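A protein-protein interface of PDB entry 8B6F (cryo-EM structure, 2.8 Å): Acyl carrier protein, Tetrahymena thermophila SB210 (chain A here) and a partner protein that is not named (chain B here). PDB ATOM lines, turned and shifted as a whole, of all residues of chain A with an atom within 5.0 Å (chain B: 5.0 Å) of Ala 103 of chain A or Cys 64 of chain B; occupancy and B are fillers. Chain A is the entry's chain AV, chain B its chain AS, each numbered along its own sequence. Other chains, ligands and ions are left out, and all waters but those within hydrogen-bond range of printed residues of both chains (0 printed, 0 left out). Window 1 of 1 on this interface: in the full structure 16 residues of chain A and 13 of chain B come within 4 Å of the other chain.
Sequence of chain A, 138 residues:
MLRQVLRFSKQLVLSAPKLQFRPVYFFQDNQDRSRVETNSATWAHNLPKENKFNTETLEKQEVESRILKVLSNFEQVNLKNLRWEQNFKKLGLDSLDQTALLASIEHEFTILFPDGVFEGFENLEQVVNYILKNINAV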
ATOM      1  N   GLN A  98     -23.977 -16.486 -17.940  1.00  0.00           N
ATOM      2  CA  GLN A  98     -22.963 -15.625 -18.546  1.00  0.00           C
ATOM      3  C   GLN A  98     -22.508 -16.164 -19.895  1.00  0.00           C
ATOM      4  O   GLN A  98     -22.392 -15.415 -20.871  1.00  0.00           O
ATOM      5  CB  GLN A  98     -21.765 -15.497 -17.605  1.00  0.00           C
ATOM      6  CG  GLN A  98     -22.057 -14.733 -16.336  1.00  0.00           C
ATOM      7  CD  GLN A  98     -20.967 -14.903 -15.300  1.00  0.00           C
ATOM      8  OE1 GLN A  98     -19.846 -15.297 -15.621  1.00  0.00           O
ATOM      9  NE2 GLN A  98     -21.294 -14.616 -14.045  1.00  0.00           N
ATOM     10  N   THR A  99     -22.242 -17.469 -19.969  1.00  0.00           N
ATOM     11  CA  THR A  99     -21.821 -18.064 -21.232  1.00  0.00           C
ATOM     12  C   THR A  99     -22.908 -17.930 -22.286  1.00  0.00           C
ATOM     13  O   THR A  99     -22.625 -17.618 -23.447  1.00  0.00           O
ATOM     14  CB  THR A  99     -21.436 -19.525 -21.010  1.00  0.00           C
ATOM     15  OG1 THR A  99     -22.508 -20.201 -20.348  1.00  0.00           O
ATOM     16  CG2 THR A  99     -20.170 -19.635 -20.174  1.00  0.00           C
ATOM     17  N   ALA A 100     -24.160 -18.177 -21.902  1.00  0.00           N
ATOM     18  CA  ALA A 100     -25.260 -18.041 -22.846  1.00  0.00           C
ATOM     19  C   ALA A 100     -25.387 -16.603 -23.330  1.00  0.00           C
ATOM     20  O   ALA A 100     -25.606 -16.356 -24.522  1.00  0.00           O
ATOM     21  CB  ALA A 100     -26.563 -18.509 -22.200  1.00  0.00           C
ATOM     22  N   LEU A 101     -25.259 -15.639 -22.416  1.00  0.00           N
ATOM     23  CA  LEU A 101     -25.373 -14.236 -22.797  1.00  0.00           C
ATOM     24  C   LEU A 101     -24.249 -13.820 -23.737  1.00  0.00           C
ATOM     25  O   LEU A 101     -24.488 -13.127 -24.732  1.00  0.00           O
ATOM     26  CB  LEU A 101     -25.368 -13.359 -21.544  1.00  0.00           C
ATOM     27  CG  LEU A 101     -25.381 -11.846 -21.770  1.00  0.00           C
ATOM     28  CD1 LEU A 101     -26.613 -11.423 -22.549  1.00  0.00           C
ATOM     29  CD2 LEU A 101     -25.308 -11.119 -20.442  1.00  0.00           C
ATOM     30  N   LEU A 102     -23.020 -14.244 -23.448  1.00  0.00           N
ATOM     31  CA  LEU A 102     -21.900 -13.900 -24.316  1.00  0.00           C
ATOM     32  C   LEU A 102     -22.049 -14.543 -25.688  1.00  0.00           C
ATOM     33  O   LEU A 102     -21.733 -13.922 -26.709  1.00  0.00           O
ATOM     34  CB  LEU A 102     -20.583 -14.310 -23.659  1.00  0.00           C
ATOM     35  CG  LEU A 102     -20.218 -13.562 -22.372  1.00  0.00           C
ATOM     36  CD1 LEU A 102     -18.905 -14.075 -21.809  1.00  0.00           C
ATOM     37  CD2 LEU A 102     -20.144 -12.059 -22.598  1.00  0.00           C
ATOM     38  N   ALA A 103     -22.524 -15.787 -25.734  1.00  0.00           N
ATOM     39  CA  ALA A 103     -22.781 -16.424 -27.020  1.00  0.00           C
ATOM     40  C   ALA A 103     -23.870 -15.685 -27.787  1.00  0.00           C
ATOM     41  O   ALA A 103     -23.780 -15.525 -29.010  1.00  0.00           O
ATOM     42  CB  ALA A 103     -23.168 -17.888 -26.813  1.00  0.00           C
ATOM     43  N   SER A 104     -24.912 -15.233 -27.087  1.00  0.00           N
ATOM     44  CA  SER A 104     -25.971 -14.476 -27.745  1.00  0.00           C
ATOM     45  C   SER A 104     -25.439 -13.165 -28.309  1.00  0.00           C
ATOM     46  O   SER A 104     -25.817 -12.755 -29.412  1.00  0.00           O
ATOM     47  CB  SER A 104     -27.112 -14.210 -26.766  1.00  0.00           C
ATOM     48  OG  SER A 104     -27.685 -15.422 -26.309  1.00  0.00           O
ATOM     49  N   ILE A 105     -24.566 -12.488 -27.561  1.00  0.00           N
ATOM     50  CA  ILE A 105     -23.971 -11.249 -28.050  1.00  0.00           C
ATOM     51  C   ILE A 105     -23.091 -11.525 -29.261  1.00  0.00           C
ATOM     52  O   ILE A 105     -23.075 -10.749 -30.223  1.00  0.00           O
ATOM     53  CB  ILE A 105     -23.192 -10.551 -26.920  1.00  0.00           C
ATOM     54  CG1 ILE A 105     -24.161 -10.084 -25.832  1.00  0.00           C
ATOM     55  CG2 ILE A 105     -22.395  -9.369 -27.461  1.00  0.00           C
ATOM     56  CD1 ILE A 105     -23.485  -9.588 -24.574  1.00  0.00           C
ATOM     57  N   GLU A 106     -22.339 -12.628 -29.235  1.00  0.00           N
ATOM     58  CA  GLU A 106     -21.551 -13.006 -30.403  1.00  0.00           C
ATOM     59  C   GLU A 106     -22.442 -13.220 -31.619  1.00  0.00           C
ATOM     60  O   GLU A 106     -22.120 -12.770 -32.723  1.00  0.00           O
ATOM     61  CB  GLU A 106     -20.748 -14.273 -30.110  1.00  0.00           C
ATOM     62  CG  GLU A 106     -19.580 -14.073 -29.164  1.00  0.00           C
ATOM     63  CD  GLU A 106     -18.793 -15.349 -28.945  1.00  0.00           C
ATOM     64  OE1 GLU A 106     -19.163 -16.384 -29.534  1.00  0.00           O
ATOM     65  OE2 GLU A 106     -17.803 -15.320 -28.187  1.00  0.00           O
ATOM     66  N   HIS A 107     -23.572 -13.905 -31.434  1.00  0.00           N
ATOM     67  CA  HIS A 107     -24.506 -14.098 -32.537  1.00  0.00           C
ATOM     68  C   HIS A 107     -25.058 -12.765 -33.022  1.00  0.00           C
ATOM     69  O   HIS A 107     -25.189 -12.541 -34.231  1.00  0.00           O
ATOM     70  CB  HIS A 107     -25.649 -15.015 -32.104  1.00  0.00           C
ATOM     71  CG  HIS A 107     -25.223 -16.420 -31.817  1.00  0.00           C
ATOM     72  ND1 HIS A 107     -24.092 -16.983 -32.368  1.00  0.00           N
ATOM     73  CD2 HIS A 107     -25.778 -17.376 -31.037  1.00  0.00           C
ATOM     74  CE1 HIS A 107     -23.968 -18.226 -31.938  1.00  0.00           C
ATOM     75  NE2 HIS A 107     -24.978 -18.490 -31.129  1.00  0.00           N
ATOM     76  N   PHE A 118     -13.111 -13.986 -23.799  1.00  0.00           N
ATOM     77  CA  PHE A 118     -14.409 -14.536 -23.421  1.00  0.00           C
ATOM     78  C   PHE A 118     -14.445 -14.874 -21.937  1.00  0.00           C
ATOM     79  O   PHE A 118     -15.416 -14.563 -21.238  1.00  0.00           O
ATOM     80  CB  PHE A 118     -14.713 -15.778 -24.262  1.00  0.00           C
ATOM     81  CG  PHE A 118     -16.127 -16.272 -24.136  1.00  0.00           C
ATOM     82  CD1 PHE A 118     -16.556 -16.909 -22.984  1.00  0.00           C
ATOM     83  CD2 PHE A 118     -17.021 -16.124 -25.181  1.00  0.00           C
ATOM     84  CE1 PHE A 118     -17.851 -17.370 -22.872  1.00  0.00           C
ATOM     85  CE2 PHE A 118     -18.318 -16.583 -25.073  1.00  0.00           C
ATOM     86  CZ  PHE A 118     -18.732 -17.206 -23.918  1.00  0.00           C
ATOM     87  N   TYR B  60     -20.450 -26.164 -22.891  1.00  0.00           N
ATOM     88  CA  TYR B  60     -21.666 -25.363 -22.950  1.00  0.00           C
ATOM     89  C   TYR B  60     -21.495 -24.183 -23.897  1.00  0.00           C
ATOM     90  O   TYR B  60     -22.432 -23.808 -24.611  1.00  0.00           O
ATOM     91  CB  TYR B  60     -22.054 -24.890 -21.551  1.00  0.00           C
ATOM     92  CG  TYR B  60     -23.415 -24.237 -21.491  1.00  0.00           C
ATOM     93  CD1 TYR B  60     -24.567 -24.953 -21.777  1.00  0.00           C
ATOM     94  CD2 TYR B  60     -23.546 -22.911 -21.142  1.00  0.00           C
ATOM     95  CE1 TYR B  60     -25.811 -24.358 -21.718  1.00  0.00           C
ATOM     96  CE2 TYR B  60     -24.781 -22.302 -21.078  1.00  0.00           C
ATOM     97  CZ  TYR B  60     -25.911 -23.031 -21.369  1.00  0.00           C
ATOM     98  OH  TYR B  60     -27.145 -22.430 -21.306  1.00  0.00           O
ATOM     99  N   ARG B  61     -20.301 -23.587 -23.919  1.00  0.00           N
ATOM    100  CA  ARG B  61     -20.036 -22.505 -24.859  1.00  0.00           C
ATOM    101  C   ARG B  61     -20.169 -22.986 -26.298  1.00  0.00           C
ATOM    102  O   ARG B  61     -20.775 -22.307 -27.132  1.00  0.00           O
ATOM    103  CB  ARG B  61     -18.638 -21.930 -24.620  1.00  0.00           C
ATOM    104  CG  ARG B  61     -18.327 -20.705 -25.464  1.00  0.00           C
ATOM    105  CD  ARG B  61     -16.875 -20.274 -25.342  1.00  0.00           C
ATOM    106  NE  ARG B  61     -16.459 -20.126 -23.951  1.00  0.00           N
ATOM    107  CZ  ARG B  61     -15.387 -20.689 -23.409  1.00  0.00           C
ATOM    108  NH1 ARG B  61     -14.557 -21.435 -24.119  1.00  0.00           N
ATOM    109  NH2 ARG B  61     -15.137 -20.494 -22.118  1.00  0.00           N
ATOM    110  N   LYS B  62     -19.612 -24.158 -26.606  1.00  0.00           N
ATOM    111  CA  LYS B  62     -19.739 -24.697 -27.954  1.00  0.00           C
ATOM    112  C   LYS B  62     -21.198 -24.967 -28.295  1.00  0.00           C
ATOM    113  O   LYS B  62     -21.648 -24.676 -29.408  1.00  0.00           O
ATOM    114  CB  LYS B  62     -18.911 -25.975 -28.086  1.00  0.00           C
ATOM    115  CG  LYS B  62     -18.770 -26.490 -29.510  1.00  0.00           C
ATOM    116  CD  LYS B  62     -18.111 -25.448 -30.401  1.00  0.00           C
ATOM    117  CE  LYS B  62     -17.615 -26.042 -31.704  1.00  0.00           C
ATOM    118  NZ  LYS B  62     -18.681 -26.740 -32.459  1.00  0.00           N
ATOM    119  N   PHE B  63     -21.949 -25.531 -27.347  1.00  0.00           N
ATOM    120  CA  PHE B  63     -23.364 -25.799 -27.581  1.00  0.00           C
ATOM    121  C   PHE B  63     -24.128 -24.510 -27.857  1.00  0.00           C
ATOM    122  O   PHE B  63     -24.970 -24.459 -28.761  1.00  0.00           O
ATOM    123  CB  PHE B  63     -23.959 -26.527 -26.376  1.00  0.00           C
ATOM    124  CG  PHE B  63     -25.454 -26.628 -26.408  1.00  0.00           C
ATOM    125  CD1 PHE B  63     -26.074 -27.687 -27.044  1.00  0.00           C
ATOM    126  CD2 PHE B  63     -26.239 -25.669 -25.792  1.00  0.00           C
ATOM    127  CE1 PHE B  63     -27.448 -27.784 -27.073  1.00  0.00           C
ATOM    128  CE2 PHE B  63     -27.615 -25.760 -25.816  1.00  0.00           C
ATOM    129  CZ  PHE B  63     -28.221 -26.819 -26.456  1.00  0.00           C
ATOM    130  N   CYS B  64     -23.849 -23.458 -27.086  1.00  0.00           N
ATOM    131  CA  CYS B  64     -24.513 -22.177 -27.305  1.00  0.00           C
ATOM    132  C   CYS B  64     -24.133 -21.577 -28.652  1.00  0.00           C
ATOM    133  O   CYS B  64     -24.977 -20.987 -29.335  1.00  0.00           O
ATOM    134  CB  CYS B  64     -24.169 -21.209 -26.174  1.00  0.00           C
ATOM    135  SG  CYS B  64     -24.891 -21.646 -24.579  1.00  0.00           S
ATOM    136  N   ARG B  65     -22.868 -21.709 -29.053  1.00  0.00           N
ATOM    137  CA  ARG B  65     -22.457 -21.194 -30.354  1.00  0.00           C
ATOM    138  C   ARG B  65     -23.108 -21.953 -31.500  1.00  0.00           C
ATOM    139  O   ARG B  65     -23.293 -21.392 -32.585  1.00  0.00           O
ATOM    140  CB  ARG B  65     -20.935 -21.260 -30.477  1.00  0.00           C
ATOM    141  CG  ARG B  65     -20.213 -20.156 -29.732  1.00  0.00           C
ATOM    142  CD  ARG B  65     -18.733 -20.456 -29.594  1.00  0.00           C
ATOM    143  NE  ARG B  65     -17.990 -19.305 -29.098  1.00  0.00           N
ATOM    144  CZ  ARG B  65     -16.736 -19.350 -28.672  1.00  0.00           C
ATOM    145  NH1 ARG B  65     -16.057 -20.484 -28.640  1.00  0.00           N
ATOM    146  NH2 ARG B  65     -16.147 -18.228 -28.270  1.00  0.00           N
ATOM    147  N   LEU B  66     -23.453 -23.223 -31.292  1.00  0.00           N
ATOM    148  CA  LEU B  66     -24.016 -24.039 -32.358  1.00  0.00           C
ATOM    149  C   LEU B  66     -25.537 -24.068 -32.382  1.00  0.00           C
ATOM    150  O   LEU B  66     -26.112 -24.448 -33.408  1.00  0.00           O
ATOM    151  CB  LEU B  66     -23.506 -25.478 -32.245  1.00  0.00           C
ATOM    152  CG  LEU B  66     -22.235 -25.817 -33.020  1.00  0.00           C
ATOM    153  CD1 LEU B  66     -21.747 -27.182 -32.600  1.00  0.00           C
ATOM    154  CD2 LEU B  66     -22.474 -25.776 -34.516  1.00  0.00           C
ATOM    155  N   ILE B  67     -26.208 -23.685 -31.292  1.00  0.00           N
ATOM    156  CA  ILE B  67     -27.657 -23.883 -31.214  1.00  0.00           C
ATOM    157  C   ILE B  67     -28.400 -23.209 -32.359  1.00  0.00           C
ATOM    158  O   ILE B  67     -29.313 -23.833 -32.918  1.00  0.00           O
ATOM    159  CB  ILE B  67     -28.176 -23.483 -29.825  1.00  0.00           C
ATOM    160  CG1 ILE B  67     -29.648 -23.876 -29.665  1.00  0.00           C
ATOM    161  CG2 ILE B  67     -28.056 -22.004 -29.582  1.00  0.00           C
ATOM    162  CD1 ILE B  67     -29.907 -25.369 -29.711  1.00  0.00           C
ATOM    163  N   PRO B  68     -28.090 -21.970 -32.769  1.00  0.00           N
ATOM    164  CA  PRO B  68     -28.888 -21.389 -33.864  1.00  0.00           C
ATOM    165  C   PRO B  68     -28.823 -22.201 -35.146  1.00  0.00           C
ATOM    166  O   PRO B  68     -29.841 -22.344 -35.835  1.00  0.00           O
ATOM    167  CB  PRO B  68     -28.285 -19.990 -34.034  1.00  0.00           C
ATOM    168  CG  PRO B  68     -26.920 -20.107 -33.515  1.00  0.00           C
ATOM    169  CD  PRO B  68     -27.006 -21.053 -32.366  1.00  0.00           C
ATOM    170  N   MET B  86     -30.927 -22.353 -25.114  1.00  0.00           N
ATOM    171  CA  MET B  86     -29.728 -22.231 -24.291  1.00  0.00           C
ATOM    172  C   MET B  86     -30.065 -22.339 -22.811  1.00  0.00           C
ATOM    173  O   MET B  86     -29.358 -23.010 -22.051  1.00  0.00           O
ATOM    174  CB  MET B  86     -29.027 -20.903 -24.574  1.00  0.00           C
ATOM    175  CG  MET B  86     -28.460 -20.775 -25.975  1.00  0.00           C
ATOM    176  SD  MET B  86     -27.762 -19.139 -26.261  1.00  0.00           S
ATOM    177  CE  MET B  86     -27.415 -19.220 -28.012  1.00  0.00           C
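The backbone carbonyl oxygen (O) of Ala 100 of chain A is in hydrogen-bond range of the side-chain hydroxyl (OG) of Ser 104 of chain A, 2.9 Å away. O of Tyr 60 of chain B is in hydrogen-bond range of SG of Cys 64 of chain B, 3.3 Å away. OH of Tyr 60 of chain B lies within hydrogen-bond range of O of Met 86 of chain B (2.4 Å).
Printed residues of chain A that touch a printed residue of chain B: Thr 99, Ala 100, Ala 103, Ser 104, Glu 106, His 107 and Phe 118. Hydrophobic or aromatic side chains of chain A within 4 Å of the printed part of chain B: Ala 103, His 107 and Phe 118. Along chain A the printed residues that touch a printed residue of chain B span positions 99 to 118. Printed residues of chain B that touch a printed residue of chain A: Tyr 60, Arg 61, Cys 64, Arg 65, Pro 68 and Met 86. Hydrophobic or aromatic side chains of chain B that line the printed part of chain A: Tyr 60, Pro 68 and Met 86. Along chain B the printed residues that touch a printed residue of chain A span positions 60 to 86. Among the printed residues, 11 pairs touch across the chains. Among the printed residues, Asp or Glu carboxylates within 4 Å of a Lys or Arg side-chain nitrogen of the other chain: Glu 106 of chain A with Arg 65 of chain B.
A ring nitrogen (NE2) of His 107 of chain A lies within hydrogen-bond range of the backbone carbonyl oxygen (O) of Cys 64 of chain B, 3.1 Å away. The side-chain carboxylate of Glu 106 of chain A lies within salt-bridge range of the guanidinium group of Arg 65 of chain B, at 3.2 Å. The side-chain sulfur (SD) of Met 86 of chain B is in hydrogen-bond range of the side-chain hydroxyl (OG) of Ser 104 of chain A, 3.7 Å away.
Gln 98 of chain A touches none of the printed residues of chain B. Of the printed residues of chain B, Thr 99 of chain A touches Tyr 60 (3.0 Å). Ala 103 of chain A touches just one residue of chain B: Cys 64. Of the printed residues of chain B, Ser 104 of chain A touches Met 86 (3.7 Å). Printed residues of chain A within 4 Å of Cys 64 of chain B: Ala 103 and His 107. Printed residues of chain A within 4 Å of Met 86 of chain B: Ala 100, Ser 104 and His 107. The nearest residue of chain B that does not touch Ala 103 of chain A is Arg 65 of chain B (4.4 Å). The nearest printed residue of chain B that does not touch His 107 of chain A is Ile 67 of chain B (4.9 Å).
Among the printed residues, pairs that only touch across the chains: Thr 99 of chain A with Tyr 60 of chain B (3.0 Å), Phe 118 of chain A with Arg 61 of chain B (3.3 Å), His 107 of chain A with Arg 65 of chain B (3.3 Å), His 107 of chain A with Pro 68 of chain B (3.5 Å), Ala 103 of chain A with Cys 64 of chain B (3.5 Å), Phe 118 of chain A with Arg 65 of chain B (3.8 Å), His 107 of chain A with Met 86 of chain B (3.9 Å) and Ala 100 of chain A with Met 86 of chain B (3.9 Å).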
